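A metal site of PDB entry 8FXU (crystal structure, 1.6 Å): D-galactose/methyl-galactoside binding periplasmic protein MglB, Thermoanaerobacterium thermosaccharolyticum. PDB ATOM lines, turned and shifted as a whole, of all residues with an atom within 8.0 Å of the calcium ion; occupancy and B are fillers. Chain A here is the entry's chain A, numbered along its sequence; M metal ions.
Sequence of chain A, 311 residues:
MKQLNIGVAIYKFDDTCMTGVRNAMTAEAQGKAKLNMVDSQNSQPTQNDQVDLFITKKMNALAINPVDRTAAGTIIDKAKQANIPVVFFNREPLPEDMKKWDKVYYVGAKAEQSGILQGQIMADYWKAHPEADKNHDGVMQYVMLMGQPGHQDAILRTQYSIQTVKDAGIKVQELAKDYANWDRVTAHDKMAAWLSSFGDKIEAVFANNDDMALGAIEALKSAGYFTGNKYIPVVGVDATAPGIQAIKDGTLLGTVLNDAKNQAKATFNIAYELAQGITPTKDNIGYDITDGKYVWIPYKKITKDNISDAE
Six residues have an atom within 4 Å of the calcium ion: Asp 133, Asn 135, Asp 137, Val 139, Gln 141 and Glu 203.
A ring nitrogen (ND1) of His 136 lies within hydrogen-bond range of the backbone carbonyl oxygen (O) of Asp 133.
The side-chain amide oxygen of Gln 173 lies within hydrogen-bond range of the side-chain amide nitrogen of Gln 141, 2.8 Å away.
The side-chain carboxylate of Glu 203 sits close to the backbone NH of Lys 134 (3.0 Å).
The side-chain carboxylate of Asp 133 sits at hydrogen-bond distance from the backbone NH of Gly 138.
The calcium ion is bound by the side-chain carboxylate (OD1) of Asp 133 (2.3 Å), the side-chain amide oxygen (OD1) of Asn 135 (2.3 Å), the backbone carbonyl oxygen (O) of Val 139 (2.3 Å), the side-chain amide oxygen (OE1) of Gln 141 (2.3 Å), the side-chain carboxylate (OD1) of Asp 137 (2.4 Å), the side-chain carboxylate (OE2) of Glu 203 (2.5 Å) and the side-chain carboxylate (OE1) of Glu 203 (2.5 Å).
The calcium ion has seven donor atoms within binding distance.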
ATOM      1  N   TRP A 126      16.621   8.558 -16.381  1.00  0.00           N
ATOM      2  CA  TRP A 126      17.945   9.151 -16.240  1.00  0.00           C
ATOM      3  C   TRP A 126      19.031   8.166 -16.690  1.00  0.00           C
ATOM      4  O   TRP A 126      19.946   8.521 -17.443  1.00  0.00           O
ATOM      5  CB  TRP A 126      18.160   9.583 -14.783  1.00  0.00           C
ATOM      6  CG  TRP A 126      19.508  10.195 -14.479  1.00  0.00           C
ATOM      7  CD1 TRP A 126      20.630   9.551 -14.041  1.00  0.00           C
ATOM      8  CD2 TRP A 126      19.850  11.582 -14.592  1.00  0.00           C
ATOM      9  NE1 TRP A 126      21.662  10.450 -13.892  1.00  0.00           N
ATOM     10  CE2 TRP A 126      21.205  11.702 -14.211  1.00  0.00           C
ATOM     11  CE3 TRP A 126      19.156  12.725 -14.983  1.00  0.00           C
ATOM     12  CZ2 TRP A 126      21.870  12.920 -14.206  1.00  0.00           C
ATOM     13  CZ3 TRP A 126      19.821  13.943 -14.978  1.00  0.00           C
ATOM     14  CH2 TRP A 126      21.167  14.026 -14.592  1.00  0.00           C
ATOM     15  N   ALA A 132      20.338  13.624 -20.627  1.00  0.00           N
ATOM     16  CA  ALA A 132      19.504  14.282 -19.602  1.00  0.00           C
ATOM     17  C   ALA A 132      20.344  15.128 -18.651  1.00  0.00           C
ATOM     18  O   ALA A 132      19.863  16.119 -18.083  1.00  0.00           O
ATOM     19  CB  ALA A 132      18.705  13.266 -18.826  1.00  0.00           C
ATOM     20  N   ASP A 133      21.592  14.723 -18.454  1.00  0.00           N
ATOM     21  CA  ASP A 133      22.526  15.464 -17.610  1.00  0.00           C
ATOM     22  C   ASP A 133      23.127  16.601 -18.436  1.00  0.00           C
ATOM     23  O   ASP A 133      24.245  16.505 -18.957  1.00  0.00           O
ATOM     24  CB  ASP A 133      23.594  14.501 -17.087  1.00  0.00           C
ATOM     25  CG  ASP A 133      24.566  15.151 -16.158  1.00  0.00           C
ATOM     26  OD1 ASP A 133      24.239  16.219 -15.604  1.00  0.00           O
ATOM     27  OD2 ASP A 133      25.660  14.566 -15.963  1.00  0.00           O
ATOM     28  N   LYS A 134      22.351  17.681 -18.559  1.00  0.00           N
ATOM     29  CA  LYS A 134      22.645  18.747 -19.511  1.00  0.00           C
ATOM     30  C   LYS A 134      23.939  19.505 -19.197  1.00  0.00           C
ATOM     31  O   LYS A 134      24.591  20.018 -20.113  1.00  0.00           O
ATOM     32  CB  LYS A 134      21.468  19.727 -19.578  1.00  0.00           C
ATOM     33  CG  LYS A 134      20.171  19.102 -20.087  1.00  0.00           C
ATOM     34  CD  LYS A 134      19.183  20.157 -20.607  1.00  0.00           C
ATOM     35  CE  LYS A 134      17.875  19.537 -21.142  1.00  0.00           C
ATOM     36  NZ  LYS A 134      16.883  19.171 -20.083  1.00  0.00           N
ATOM     37  N   ASN A 135      24.329  19.569 -17.927  1.00  0.00           N
ATOM     38  CA  ASN A 135      25.584  20.260 -17.599  1.00  0.00           C
ATOM     39  C   ASN A 135      26.729  19.273 -17.316  1.00  0.00           C
ATOM     40  O   ASN A 135      27.801  19.679 -16.887  1.00  0.00           O
ATOM     41  CB  ASN A 135      25.372  21.206 -16.398  1.00  0.00           C
ATOM     42  CG  ASN A 135      25.259  20.468 -15.077  1.00  0.00           C
ATOM     43  OD1 ASN A 135      24.853  19.316 -15.035  1.00  0.00           O
ATOM     44  ND2 ASN A 135      25.629  21.148 -13.989  1.00  0.00           N
ATOM     45  N   HIS A 136      26.483  17.995 -17.577  1.00  0.00           N
ATOM     46  CA  HIS A 136      27.527  16.963 -17.539  1.00  0.00           C
ATOM     47  C   HIS A 136      28.292  16.869 -16.218  1.00  0.00           C
ATOM     48  O   HIS A 136      29.495  16.563 -16.226  1.00  0.00           O
ATOM     49  CB  HIS A 136      28.539  17.206 -18.674  1.00  0.00           C
ATOM     50  CG  HIS A 136      27.900  17.532 -19.988  1.00  0.00           C
ATOM     51  ND1 HIS A 136      27.206  16.598 -20.736  1.00  0.00           N
ATOM     52  CD2 HIS A 136      27.847  18.687 -20.687  1.00  0.00           C
ATOM     53  CE1 HIS A 136      26.757  17.162 -21.840  1.00  0.00           C
ATOM     54  NE2 HIS A 136      27.132  18.430 -21.841  1.00  0.00           N
ATOM     55  N   ASP A 137      27.616  17.124 -15.105  1.00  0.00           N
ATOM     56  CA  ASP A 137      28.278  17.076 -13.809  1.00  0.00           C
ATOM     57  C   ASP A 137      28.021  15.772 -13.046  1.00  0.00           C
ATOM     58  O   ASP A 137      28.508  15.598 -11.929  1.00  0.00           O
ATOM     59  CB  ASP A 137      27.876  18.285 -12.940  1.00  0.00           C
ATOM     60  CG  ASP A 137      26.401  18.290 -12.561  1.00  0.00           C
ATOM     61  OD1 ASP A 137      25.621  17.432 -13.031  1.00  0.00           O
ATOM     62  OD2 ASP A 137      26.020  19.182 -11.764  1.00  0.00           O
ATOM     63  N   GLY A 138      27.262  14.861 -13.652  1.00  0.00           N
ATOM     64  CA  GLY A 138      26.944  13.588 -13.037  1.00  0.00           C
ATOM     65  C   GLY A 138      25.953  13.687 -11.883  1.00  0.00           C
ATOM     66  O   GLY A 138      25.869  12.795 -11.039  1.00  0.00           O
ATOM     67  N   VAL A 139      25.203  14.783 -11.859  1.00  0.00           N
ATOM     68  CA  VAL A 139      24.202  15.054 -10.819  1.00  0.00           C
ATOM     69  C   VAL A 139      22.894  15.446 -11.492  1.00  0.00           C
ATOM     70  O   VAL A 139      22.895  16.228 -12.445  1.00  0.00           O
ATOM     71  CB  VAL A 139      24.676  16.159  -9.860  1.00  0.00           C
ATOM     72  CG1 VAL A 139      23.633  16.410  -8.775  1.00  0.00           C
ATOM     73  CG2 VAL A 139      26.019  15.798  -9.236  1.00  0.00           C
ATOM     74  N   MET A 140      21.770  14.926 -11.005  1.00  0.00           N
ATOM     75  CA  MET A 140      20.464  15.336 -11.504  1.00  0.00           C
ATOM     76  C   MET A 140      19.971  16.600 -10.820  1.00  0.00           C
ATOM     77  O   MET A 140      19.587  16.575  -9.649  1.00  0.00           O
ATOM     78  CB  MET A 140      19.444  14.205 -11.315  1.00  0.00           C
ATOM     79  CG  MET A 140      18.027  14.577 -11.725  1.00  0.00           C
ATOM     80  SD  MET A 140      16.776  13.416 -11.073  1.00  0.00           S
ATOM     81  CE  MET A 140      17.165  11.938 -12.013  1.00  0.00           C
ATOM     82  N   GLN A 141      19.984  17.718 -11.548  1.00  0.00           N
ATOM     83  CA  GLN A 141      19.401  18.963 -11.024  1.00  0.00           C
ATOM     84  C   GLN A 141      17.888  18.936 -11.179  1.00  0.00           C
ATOM     85  O   GLN A 141      17.402  18.855 -12.309  1.00  0.00           O
ATOM     86  CB  GLN A 141      19.945  20.179 -11.763  1.00  0.00           C
ATOM     87  CG  GLN A 141      21.256  20.733 -11.210  1.00  0.00           C
ATOM     88  CD  GLN A 141      22.459  19.891 -11.584  1.00  0.00           C
ATOM     89  OE1 GLN A 141      22.566  19.383 -12.703  1.00  0.00           O
ATOM     90  NE2 GLN A 141      23.410  19.780 -10.652  1.00  0.00           N
ATOM     91  N   TYR A 142      17.152  19.052 -10.072  1.00  0.00           N
ATOM     92  CA  TYR A 142      15.699  18.960 -10.156  1.00  0.00           C
ATOM     93  C   TYR A 142      14.981  20.079  -9.407  1.00  0.00           C
ATOM     94  O   TYR A 142      15.564  20.758  -8.560  1.00  0.00           O
ATOM     95  CB  TYR A 142      15.216  17.600  -9.608  1.00  0.00           C
ATOM     96  CG  TYR A 142      15.304  17.461  -8.100  1.00  0.00           C
ATOM     97  CD1 TYR A 142      16.453  16.970  -7.491  1.00  0.00           C
ATOM     98  CD2 TYR A 142      14.222  17.810  -7.278  1.00  0.00           C
ATOM     99  CE1 TYR A 142      16.548  16.847  -6.109  1.00  0.00           C
ATOM    100  CE2 TYR A 142      14.300  17.683  -5.872  1.00  0.00           C
ATOM    101  CZ  TYR A 142      15.469  17.182  -5.314  1.00  0.00           C
ATOM    102  OH  TYR A 142      15.595  17.063  -3.952  1.00  0.00           O
ATOM    103  N   LYS A 171      23.146  10.759  -8.058  1.00  0.00           N
ATOM    104  CA  LYS A 171      23.348  11.955  -7.245  1.00  0.00           C
ATOM    105  C   LYS A 171      22.364  13.018  -7.671  1.00  0.00           C
ATOM    106  O   LYS A 171      22.092  13.198  -8.865  1.00  0.00           O
ATOM    107  CB  LYS A 171      24.779  12.476  -7.375  1.00  0.00           C
ATOM    108  CG  LYS A 171      25.830  11.527  -6.826  1.00  0.00           C
ATOM    109  CD  LYS A 171      27.226  12.102  -7.064  1.00  0.00           C
ATOM    110  CE  LYS A 171      28.323  11.132  -6.671  1.00  0.00           C
ATOM    111  NZ  LYS A 171      29.650  11.648  -7.077  1.00  0.00           N
ATOM    112  N   GLN A 173      20.550  17.137  -6.989  1.00  0.00           N
ATOM    113  CA  GLN A 173      20.660  18.481  -6.454  1.00  0.00           C
ATOM    114  C   GLN A 173      19.336  19.183  -6.606  1.00  0.00           C
ATOM    115  O   GLN A 173      18.841  19.363  -7.718  1.00  0.00           O
ATOM    116  CB  GLN A 173      21.753  19.290  -7.168  1.00  0.00           C
ATOM    117  CG  GLN A 173      21.898  20.669  -6.564  1.00  0.00           C
ATOM    118  CD  GLN A 173      22.964  21.500  -7.231  1.00  0.00           C
ATOM    119  OE1 GLN A 173      23.111  21.478  -8.455  1.00  0.00           O
ATOM    120  NE2 GLN A 173      23.725  22.237  -6.429  1.00  0.00           N
ATOM    121  N   ASP A 200      18.033  26.735 -18.182  1.00  0.00           N
ATOM    122  CA  ASP A 200      18.439  25.422 -18.672  1.00  0.00           C
ATOM    123  C   ASP A 200      19.209  24.630 -17.621  1.00  0.00           C
ATOM    124  O   ASP A 200      19.689  23.543 -17.901  1.00  0.00           O
ATOM    125  CB  ASP A 200      19.271  25.537 -19.946  1.00  0.00           C
ATOM    126  CG  ASP A 200      19.253  24.248 -20.769  1.00  0.00           C
ATOM    127  OD1 ASP A 200      18.148  23.678 -20.954  1.00  0.00           O
ATOM    128  OD2 ASP A 200      20.332  23.806 -21.215  1.00  0.00           O
ATOM    129  N   LYS A 201      19.289  25.148 -16.395  1.00  0.00           N
ATOM    130  CA  LYS A 201      19.900  24.359 -15.321  1.00  0.00           C
ATOM    131  C   LYS A 201      18.991  23.211 -14.864  1.00  0.00           C
ATOM    132  O   LYS A 201      19.476  22.207 -14.350  1.00  0.00           O
ATOM    133  CB  LYS A 201      20.231  25.222 -14.099  1.00  0.00           C
ATOM    134  CG  LYS A 201      21.422  26.144 -14.273  1.00  0.00           C
ATOM    135  CD  LYS A 201      21.735  26.812 -12.936  1.00  0.00           C
ATOM    136  CE  LYS A 201      23.096  27.472 -12.980  1.00  0.00           C
ATOM    137  NZ  LYS A 201      24.177  26.485 -13.318  1.00  0.00           N
ATOM    138  N   ILE A 202      17.679  23.380 -15.050  1.00  0.00           N
ATOM    139  CA  ILE A 202      16.724  22.389 -14.584  1.00  0.00           C
ATOM    140  C   ILE A 202      16.771  21.151 -15.474  1.00  0.00           C
ATOM    141  O   ILE A 202      16.600  21.265 -16.693  1.00  0.00           O
ATOM    142  CB  ILE A 202      15.295  22.959 -14.541  1.00  0.00           C
ATOM    143  CG1 ILE A 202      15.258  24.257 -13.731  1.00  0.00           C
ATOM    144  CG2 ILE A 202      14.345  21.921 -13.937  1.00  0.00           C
ATOM    145  CD1 ILE A 202      13.879  24.938 -13.714  1.00  0.00           C
ATOM    146  N   GLU A 203      16.978  19.988 -14.874  1.00  0.00           N
ATOM    147  CA  GLU A 203      17.111  18.752 -15.637  1.00  0.00           C
ATOM    148  C   GLU A 203      15.957  17.786 -15.416  1.00  0.00           C
ATOM    149  O   GLU A 203      15.783  16.831 -16.168  1.00  0.00           O
ATOM    150  CB  GLU A 203      18.444  18.072 -15.306  1.00  0.00           C
ATOM    151  CG  GLU A 203      19.646  18.919 -15.725  1.00  0.00           C
ATOM    152  CD  GLU A 203      20.989  18.364 -15.267  1.00  0.00           C
ATOM    153  OE1 GLU A 203      21.017  17.442 -14.422  1.00  0.00           O
ATOM    154  OE2 GLU A 203      22.034  18.839 -15.767  1.00  0.00           O
HETATM  155 CA    CA M   1      23.458  17.738 -14.095  1.00  0.00          CA
